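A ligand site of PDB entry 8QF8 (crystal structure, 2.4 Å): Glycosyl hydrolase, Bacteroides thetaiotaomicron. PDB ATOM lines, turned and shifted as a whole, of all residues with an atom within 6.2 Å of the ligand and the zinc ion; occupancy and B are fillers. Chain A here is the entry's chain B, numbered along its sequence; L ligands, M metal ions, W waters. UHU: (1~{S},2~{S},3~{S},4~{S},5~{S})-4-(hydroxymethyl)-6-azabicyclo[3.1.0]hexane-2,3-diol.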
ATOM      1  N   TRP A  79       8.370  -2.017 -11.316  1.00  0.00           N
ATOM      2  CA  TRP A  79       8.967  -2.020  -9.988  1.00  0.00           C
ATOM      3  C   TRP A  79       8.538  -3.245  -9.181  1.00  0.00           C
ATOM      4  O   TRP A  79       9.155  -3.540  -8.160  1.00  0.00           O
ATOM      5  CB  TRP A  79       8.585  -0.738  -9.228  1.00  0.00           C
ATOM      6  CG  TRP A  79       9.081   0.546  -9.844  1.00  0.00           C
ATOM      7  CD1 TRP A  79       9.643   0.769 -11.064  1.00  0.00           C
ATOM      8  CD2 TRP A  79       9.042   1.827  -9.180  1.00  0.00           C
ATOM      9  NE1 TRP A  79       9.936   2.104 -11.220  1.00  0.00           N
ATOM     10  CE2 TRP A  79       9.591   2.775 -10.081  1.00  0.00           C
ATOM     11  CE3 TRP A  79       8.617   2.251  -7.927  1.00  0.00           C
ATOM     12  CZ2 TRP A  79       9.717   4.116  -9.743  1.00  0.00           C
ATOM     13  CZ3 TRP A  79       8.758   3.585  -7.594  1.00  0.00           C
ATOM     14  CH2 TRP A  79       9.309   4.502  -8.487  1.00  0.00           C
ATOM     15  N   LEU A  84      10.861  -3.622  -5.570  1.00  0.00           N
ATOM     16  CA  LEU A  84       9.770  -3.100  -4.747  1.00  0.00           C
ATOM     17  C   LEU A  84       8.534  -3.995  -4.815  1.00  0.00           C
ATOM     18  O   LEU A  84       7.434  -3.549  -4.519  1.00  0.00           O
ATOM     19  CB  LEU A  84       9.478  -1.643  -5.151  1.00  0.00           C
ATOM     20  CG  LEU A  84      10.122  -0.594  -4.251  1.00  0.00           C
ATOM     21  CD1 LEU A  84       9.947   0.813  -4.829  1.00  0.00           C
ATOM     22  CD2 LEU A  84       9.555  -0.661  -2.827  1.00  0.00           C
ATOM     23  N   PHE A 154      18.673   4.312   0.148  1.00  0.00           N
ATOM     24  CA  PHE A 154      17.529   3.672  -0.482  1.00  0.00           C
ATOM     25  C   PHE A 154      17.696   2.151  -0.503  1.00  0.00           C
ATOM     26  O   PHE A 154      17.088   1.478  -1.339  1.00  0.00           O
ATOM     27  CB  PHE A 154      17.329   4.221  -1.896  1.00  0.00           C
ATOM     28  CG  PHE A 154      18.484   3.984  -2.837  1.00  0.00           C
ATOM     29  CD1 PHE A 154      19.589   4.831  -2.831  1.00  0.00           C
ATOM     30  CD2 PHE A 154      18.468   2.914  -3.735  1.00  0.00           C
ATOM     31  CE1 PHE A 154      20.650   4.611  -3.692  1.00  0.00           C
ATOM     32  CE2 PHE A 154      19.546   2.697  -4.586  1.00  0.00           C
ATOM     33  CZ  PHE A 154      20.632   3.550  -4.567  1.00  0.00           C
ATOM     34  N   TRP A 160      15.708  -3.019  -2.077  1.00  0.00           N
ATOM     35  CA  TRP A 160      15.241  -1.686  -2.431  1.00  0.00           C
ATOM     36  C   TRP A 160      14.166  -1.238  -1.440  1.00  0.00           C
ATOM     37  O   TRP A 160      13.051  -1.759  -1.447  1.00  0.00           O
ATOM     38  CB  TRP A 160      14.744  -1.718  -3.884  1.00  0.00           C
ATOM     39  CG  TRP A 160      14.412  -0.367  -4.472  1.00  0.00           C
ATOM     40  CD1 TRP A 160      14.761   0.867  -4.013  1.00  0.00           C
ATOM     41  CD2 TRP A 160      13.627  -0.134  -5.669  1.00  0.00           C
ATOM     42  NE1 TRP A 160      14.254   1.847  -4.817  1.00  0.00           N
ATOM     43  CE2 TRP A 160      13.560   1.273  -5.851  1.00  0.00           C
ATOM     44  CE3 TRP A 160      12.969  -0.960  -6.587  1.00  0.00           C
ATOM     45  CZ2 TRP A 160      12.863   1.850  -6.916  1.00  0.00           C
ATOM     46  CZ3 TRP A 160      12.296  -0.388  -7.652  1.00  0.00           C
ATOM     47  CH2 TRP A 160      12.237   0.999  -7.799  1.00  0.00           C
ATOM     48  N   VAL A 161      14.528  -0.273  -0.562  1.00  0.00           N
ATOM     49  CA  VAL A 161      13.679   0.391   0.419  1.00  0.00           C
ATOM     50  C   VAL A 161      12.634  -0.556   1.019  1.00  0.00           C
ATOM     51  O   VAL A 161      11.431  -0.285   0.975  1.00  0.00           O
ATOM     52  CB  VAL A 161      13.059   1.696  -0.132  1.00  0.00           C
ATOM     53  CG1 VAL A 161      14.130   2.731  -0.433  1.00  0.00           C
ATOM     54  CG2 VAL A 161      12.191   1.490  -1.370  1.00  0.00           C
ATOM     55  N   TYR A 164      10.045   1.066   3.442  1.00  0.00           N
ATOM     56  CA  TYR A 164       9.038   1.798   2.672  1.00  0.00           C
ATOM     57  C   TYR A 164       7.989   0.829   2.121  1.00  0.00           C
ATOM     58  O   TYR A 164       6.808   1.165   2.098  1.00  0.00           O
ATOM     59  CB  TYR A 164       9.709   2.616   1.554  1.00  0.00           C
ATOM     60  CG  TYR A 164       8.804   3.258   0.506  1.00  0.00           C
ATOM     61  CD1 TYR A 164       8.273   2.517  -0.550  1.00  0.00           C
ATOM     62  CD2 TYR A 164       8.491   4.611   0.562  1.00  0.00           C
ATOM     63  CE1 TYR A 164       7.451   3.102  -1.496  1.00  0.00           C
ATOM     64  CE2 TYR A 164       7.667   5.205  -0.384  1.00  0.00           C
ATOM     65  CZ  TYR A 164       7.151   4.457  -1.422  1.00  0.00           C
ATOM     66  OH  TYR A 164       6.352   5.077  -2.339  1.00  0.00           O
ATOM     67  N   GLU A 215      15.160   4.689   3.380  1.00  0.00           N
ATOM     68  CA  GLU A 215      13.822   5.240   3.265  1.00  0.00           C
ATOM     69  C   GLU A 215      12.823   4.203   3.772  1.00  0.00           C
ATOM     70  O   GLU A 215      12.883   3.041   3.365  1.00  0.00           O
ATOM     71  CB  GLU A 215      13.502   5.618   1.818  1.00  0.00           C
ATOM     72  CG  GLU A 215      12.111   6.210   1.636  1.00  0.00           C
ATOM     73  CD  GLU A 215      11.695   6.545   0.213  1.00  0.00           C
ATOM     74  OE1 GLU A 215      12.452   6.217  -0.730  1.00  0.00           O
ATOM     75  OE2 GLU A 215      10.613   7.145   0.055  1.00  0.00           O
ATOM     76  N   HIS A 262      16.032  13.946  -0.568  1.00  0.00           N
ATOM     77  CA  HIS A 262      14.928  13.341  -1.307  1.00  0.00           C
ATOM     78  C   HIS A 262      13.642  13.656  -0.536  1.00  0.00           C
ATOM     79  O   HIS A 262      13.546  13.326   0.635  1.00  0.00           O
ATOM     80  CB  HIS A 262      15.208  11.851  -1.504  1.00  0.00           C
ATOM     81  CG  HIS A 262      14.159  11.158  -2.309  1.00  0.00           C
ATOM     82  ND1 HIS A 262      13.010  10.710  -1.709  1.00  0.00           N
ATOM     83  CD2 HIS A 262      14.057  10.821  -3.604  1.00  0.00           C
ATOM     84  CE1 HIS A 262      12.241  10.146  -2.610  1.00  0.00           C
ATOM     85  NE2 HIS A 262      12.842  10.191  -3.769  1.00  0.00           N
ATOM     86  N   ASN A 264      10.089  13.064  -0.911  1.00  0.00           N
ATOM     87  CA  ASN A 264       9.038  12.133  -0.538  1.00  0.00           C
ATOM     88  C   ASN A 264       9.493  11.182   0.561  1.00  0.00           C
ATOM     89  O   ASN A 264       8.655  10.587   1.242  1.00  0.00           O
ATOM     90  CB  ASN A 264       8.516  11.307  -1.727  1.00  0.00           C
ATOM     91  CG  ASN A 264       7.127  10.745  -1.472  1.00  0.00           C
ATOM     92  OD1 ASN A 264       6.201  11.465  -1.112  1.00  0.00           O
ATOM     93  ND2 ASN A 264       6.960   9.439  -1.599  1.00  0.00           N
ATOM     94  N   THR A 265      10.815  11.015   0.750  1.00  0.00           N
ATOM     95  CA  THR A 265      11.345  10.295   1.900  1.00  0.00           C
ATOM     96  C   THR A 265      10.925  10.995   3.187  1.00  0.00           C
ATOM     97  O   THR A 265      10.524  10.316   4.137  1.00  0.00           O
ATOM     98  CB  THR A 265      12.871  10.113   1.806  1.00  0.00           C
ATOM     99  OG1 THR A 265      13.160   9.285   0.682  1.00  0.00           O
ATOM    100  CG2 THR A 265      13.489   9.482   3.037  1.00  0.00           C
ATOM    101  N   GLU A 318      12.790  14.671  -7.742  1.00  0.00           N
ATOM    102  CA  GLU A 318      12.436  14.053  -6.475  1.00  0.00           C
ATOM    103  C   GLU A 318      13.122  14.700  -5.263  1.00  0.00           C
ATOM    104  O   GLU A 318      12.918  14.224  -4.158  1.00  0.00           O
ATOM    105  CB  GLU A 318      12.727  12.549  -6.476  1.00  0.00           C
ATOM    106  CG  GLU A 318      12.193  11.803  -7.693  1.00  0.00           C
ATOM    107  CD  GLU A 318      12.325  10.300  -7.593  1.00  0.00           C
ATOM    108  OE1 GLU A 318      12.832   9.815  -6.555  1.00  0.00           O
ATOM    109  OE2 GLU A 318      11.903   9.612  -8.551  1.00  0.00           O
ATOM    110  N   GLU A 337       6.915  15.822  -7.989  1.00  0.00           N
ATOM    111  CA  GLU A 337       6.399  14.470  -7.905  1.00  0.00           C
ATOM    112  C   GLU A 337       5.028  14.482  -7.224  1.00  0.00           C
ATOM    113  O   GLU A 337       4.828  15.245  -6.280  1.00  0.00           O
ATOM    114  CB  GLU A 337       7.392  13.582  -7.156  1.00  0.00           C
ATOM    115  CG  GLU A 337       6.898  12.160  -6.980  1.00  0.00           C
ATOM    116  CD  GLU A 337       7.762  11.259  -6.117  1.00  0.00           C
ATOM    117  OE1 GLU A 337       7.240  10.213  -5.717  1.00  0.00           O
ATOM    118  OE2 GLU A 337       8.927  11.608  -5.839  1.00  0.00           O
ATOM    119  N   THR A 338       4.099  13.619  -7.674  1.00  0.00           N
ATOM    120  CA  THR A 338       2.725  13.626  -7.177  1.00  0.00           C
ATOM    121  C   THR A 338       2.630  13.082  -5.755  1.00  0.00           C
ATOM    122  O   THR A 338       1.872  13.630  -4.960  1.00  0.00           O
ATOM    123  CB  THR A 338       1.771  12.877  -8.112  1.00  0.00           C
ATOM    124  OG1 THR A 338       2.156  13.126  -9.464  1.00  0.00           O
ATOM    125  CG2 THR A 338       0.329  13.301  -7.926  1.00  0.00           C
ATOM    126  N   CYS A 339       3.404  12.036  -5.414  1.00  0.00           N
ATOM    127  CA  CYS A 339       3.412  11.487  -4.053  1.00  0.00           C
ATOM    128  C   CYS A 339       3.619  12.585  -3.007  1.00  0.00           C
ATOM    129  O   CYS A 339       2.987  12.547  -1.942  1.00  0.00           O
ATOM    130  CB  CYS A 339       4.503  10.435  -3.845  1.00  0.00           C
ATOM    131  SG  CYS A 339       4.190   8.862  -4.621  1.00  0.00           S
ATOM    132  N   ASN A 340       4.503  13.536  -3.292  1.00  0.00           N
ATOM    133  CA  ASN A 340       4.867  14.581  -2.344  1.00  0.00           C
ATOM    134  C   ASN A 340       3.632  15.404  -1.968  1.00  0.00           C
ATOM    135  O   ASN A 340       3.438  15.709  -0.795  1.00  0.00           O
ATOM    136  CB  ASN A 340       5.985  15.480  -2.868  1.00  0.00           C
ATOM    137  CG  ASN A 340       7.192  14.739  -3.416  1.00  0.00           C
ATOM    138  OD1 ASN A 340       7.104  13.549  -3.711  1.00  0.00           O
ATOM    139  ND2 ASN A 340       8.296  15.439  -3.604  1.00  0.00           N
ATOM    140  N   TYR A 393       3.459  10.918 -12.638  1.00  0.00           N
ATOM    141  CA  TYR A 393       4.547  10.896 -11.673  1.00  0.00           C
ATOM    142  C   TYR A 393       5.145  12.291 -11.561  1.00  0.00           C
ATOM    143  O   TYR A 393       5.193  12.848 -10.464  1.00  0.00           O
ATOM    144  CB  TYR A 393       5.544   9.815 -12.109  1.00  0.00           C
ATOM    145  CG  TYR A 393       6.653   9.378 -11.151  1.00  0.00           C
ATOM    146  CD1 TYR A 393       7.558  10.272 -10.583  1.00  0.00           C
ATOM    147  CD2 TYR A 393       6.860   8.030 -10.887  1.00  0.00           C
ATOM    148  CE1 TYR A 393       8.593   9.853  -9.752  1.00  0.00           C
ATOM    149  CE2 TYR A 393       7.895   7.591 -10.070  1.00  0.00           C
ATOM    150  CZ  TYR A 393       8.771   8.510  -9.502  1.00  0.00           C
ATOM    151  OH  TYR A 393       9.798   8.069  -8.689  1.00  0.00           O
ATOM    152  N   TRP A 413       4.613   2.395 -10.282  1.00  0.00           N
ATOM    153  CA  TRP A 413       5.383   3.451  -9.634  1.00  0.00           C
ATOM    154  C   TRP A 413       4.770   3.776  -8.277  1.00  0.00           C
ATOM    155  O   TRP A 413       3.601   3.501  -8.046  1.00  0.00           O
ATOM    156  CB  TRP A 413       5.432   4.733 -10.468  1.00  0.00           C
ATOM    157  CG  TRP A 413       5.618   4.541 -11.945  1.00  0.00           C
ATOM    158  CD1 TRP A 413       6.398   3.633 -12.580  1.00  0.00           C
ATOM    159  CD2 TRP A 413       4.976   5.313 -12.975  1.00  0.00           C
ATOM    160  NE1 TRP A 413       6.277   3.766 -13.937  1.00  0.00           N
ATOM    161  CE2 TRP A 413       5.424   4.792 -14.209  1.00  0.00           C
ATOM    162  CE3 TRP A 413       4.080   6.392 -12.976  1.00  0.00           C
ATOM    163  CZ2 TRP A 413       4.996   5.312 -15.427  1.00  0.00           C
ATOM    164  CZ3 TRP A 413       3.672   6.906 -14.185  1.00  0.00           C
ATOM    165  CH2 TRP A 413       4.105   6.359 -15.385  1.00  0.00           C
ATOM    166  N   CYS A 414       5.555   4.481  -7.459  1.00  0.00           N
ATOM    167  CA  CYS A 414       5.057   5.083  -6.227  1.00  0.00           C
ATOM    168  C   CYS A 414       3.850   5.988  -6.505  1.00  0.00           C
ATOM    169  O   CYS A 414       2.880   5.965  -5.760  1.00  0.00           O
ATOM    170  CB  CYS A 414       6.161   5.896  -5.547  1.00  0.00           C
ATOM    171  SG  CYS A 414       6.927   7.064  -6.654  1.00  0.00           S
ATOM    172  N   CYS A 415       3.923   6.771  -7.596  1.00  0.00           N
ATOM    173  CA  CYS A 415       2.886   7.727  -7.950  1.00  0.00           C
ATOM    174  C   CYS A 415       1.631   7.040  -8.508  1.00  0.00           C
ATOM    175  O   CYS A 415       0.586   7.684  -8.516  1.00  0.00           O
ATOM    176  CB  CYS A 415       3.481   8.759  -8.905  1.00  0.00           C
ATOM    177  SG  CYS A 415       4.579   9.904  -8.086  1.00  0.00           S
ATOM    178  N   VAL A 416       1.721   5.773  -8.950  1.00  0.00           N
ATOM    179  CA  VAL A 416       0.539   4.968  -9.215  1.00  0.00           C
ATOM    180  C   VAL A 416      -0.140   4.602  -7.896  1.00  0.00           C
ATOM    181  O   VAL A 416      -1.347   4.804  -7.736  1.00  0.00           O
ATOM    182  CB  VAL A 416       0.872   3.708 -10.042  1.00  0.00           C
ATOM    183  CG1 VAL A 416      -0.329   2.793 -10.187  1.00  0.00           C
ATOM    184  CG2 VAL A 416       1.443   4.071 -11.396  1.00  0.00           C
ATOM    185  N   SER A 418       0.014   6.016  -4.775  1.00  0.00           N
ATOM    186  CA  SER A 418      -0.662   7.165  -4.209  1.00  0.00           C
ATOM    187  C   SER A 418      -1.783   7.651  -5.143  1.00  0.00           C
ATOM    188  O   SER A 418      -2.776   8.187  -4.675  1.00  0.00           O
ATOM    189  CB  SER A 418       0.333   8.265  -3.927  1.00  0.00           C
ATOM    190  OG  SER A 418       1.079   8.599  -5.081  1.00  0.00           O
ATOM    191  N   GLN A 686      18.468   8.573  -5.878  1.00  0.00           N
ATOM    192  CA  GLN A 686      18.135   7.165  -5.663  1.00  0.00           C
ATOM    193  C   GLN A 686      17.429   6.565  -6.878  1.00  0.00           C
ATOM    194  O   GLN A 686      17.795   5.473  -7.299  1.00  0.00           O
ATOM    195  CB  GLN A 686      17.372   6.945  -4.352  1.00  0.00           C
ATOM    196  CG  GLN A 686      16.092   7.756  -4.206  1.00  0.00           C
ATOM    197  CD  GLN A 686      15.473   7.526  -2.857  1.00  0.00           C
ATOM    198  OE1 GLN A 686      16.082   7.762  -1.816  1.00  0.00           O
ATOM    199  NE2 GLN A 686      14.239   7.040  -2.874  1.00  0.00           N
ATOM    200  N   GLN A 687      16.458   7.278  -7.472  1.00  0.00           N
ATOM    201  CA  GLN A 687      15.668   6.715  -8.566  1.00  0.00           C
ATOM    202  C   GLN A 687      16.468   6.605  -9.863  1.00  0.00           C
ATOM    203  O   GLN A 687      16.438   5.542 -10.483  1.00  0.00           O
ATOM    204  CB  GLN A 687      14.342   7.466  -8.759  1.00  0.00           C
ATOM    205  CG  GLN A 687      13.256   6.637  -9.444  1.00  0.00           C
ATOM    206  CD  GLN A 687      13.007   5.324  -8.741  1.00  0.00           C
ATOM    207  OE1 GLN A 687      12.839   5.303  -7.514  1.00  0.00           O
ATOM    208  NE2 GLN A 687      13.016   4.223  -9.482  1.00  0.00           N
HETATM  209  N1  UHU L   1      11.270   6.839  -5.612  1.00  0.00           N
HETATM  210  C1  UHU L   1      10.022   6.117  -5.172  1.00  0.00           C
HETATM  211  C2  UHU L   1       9.962   7.565  -5.572  1.00  0.00           C
HETATM  212  C3  UHU L   1       9.686   8.382  -4.341  1.00  0.00           C
HETATM  213  O1  UHU L   1      10.383   9.587  -4.593  1.00  0.00           O
HETATM  214  C4  UHU L   1      10.101   7.482  -3.187  1.00  0.00           C
HETATM  215  O2  UHU L   1       9.424   7.787  -1.979  1.00  0.00           O
HETATM  216  C5  UHU L   1       9.738   6.072  -3.680  1.00  0.00           C
HETATM  217  C6  UHU L   1      10.479   4.943  -2.972  1.00  0.00           C
HETATM  218  O3  UHU L   1      11.889   5.060  -2.989  1.00  0.00           O
HETATM  219 ZN    ZN M   1       5.773   8.997  -6.362  1.00  0.00          ZN
HETATM  220  O   HOH W   1      13.964   4.852  -4.904  1.00  0.00           O
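Water W1 lies within hydrogen-bond range of O3 of the ligand (2.8 Å), OE1 of Gln 687 (2.9 Å), NE2 of Gln 686 (3.0 Å) and NE1 of Trp 160 (3.0 Å).
The side-chain sulfur (SG) of Cys 415 sits close to the backbone NH (N) of Thr 338.
The side-chain amide oxygen (OD1) of Asn 340 lies close to the side-chain carboxylate (OE2) of Glu 337, 3.4 Å away.
OD1 of Asn 264 sits close to OD1 of Asn 340 (3.5 Å).
OE2 of Glu 215 lies close to OG1 of Thr 265.
N of Leu 84 lies within hydrogen-bond range of O of Trp 79 (3.1 Å).
OD1 of Asn 264 lies close to O of Cys 339, at 3.5 Å.
The side-chain carboxylate of Glu 318 is in hydrogen-bond range of a ring nitrogen (NE2) of His 262 (2.8 Å).
The side-chain carboxylate of Glu 318 is in hydrogen-bond range of the side-chain hydroxyl of Tyr 393, at 2.6 Å.
OE1 of Glu 337 binds the zinc ion (2.0 Å).
The zinc ion is bound by SG of Cys 414 (2.3 Å).
The side-chain sulfur (SG) of Cys 415 is bound to the zinc ion (2.3 Å).
The zinc ion is bound by the side-chain sulfur (SG) of Cys 339.
The zinc ion has four donor atoms within binding distance.
O1 of the ligand is in hydrogen-bond range of NE2 of His 262 (2.7 Å).
A nitrogen (N1) of the ligand is in hydrogen-bond range of the side-chain amide oxygen of Gln 687.
OE2 of Glu 337 sits at hydrogen-bond distance from O1 of the ligand, at 2.8 Å.
OE1 of Glu 318 lies within salt-bridge range of N1 of the ligand (3.5 Å).
An oxygen (O2) of the ligand sits at hydrogen-bond distance from the side-chain carboxylate (OE2) of Glu 215 (2.4 Å).
NE2 of Gln 686 sits at hydrogen-bond distance from O3 of the ligand (3.1 Å).
O2 of the ligand lies within hydrogen-bond range of ND2 of Asn 264 (3.0 Å).
Merely in contact with the ligand: Tyr 393 (3.2 Å), Tyr 164 (3.5 Å), Trp 79 (3.7 Å) and Val 161 (3.9 Å).
The nearest printed residue that does not touch the ligand is Trp 160 (4.4 Å).
The nearest printed residue that does not touch the zinc ion is Tyr 393 (4.4 Å).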
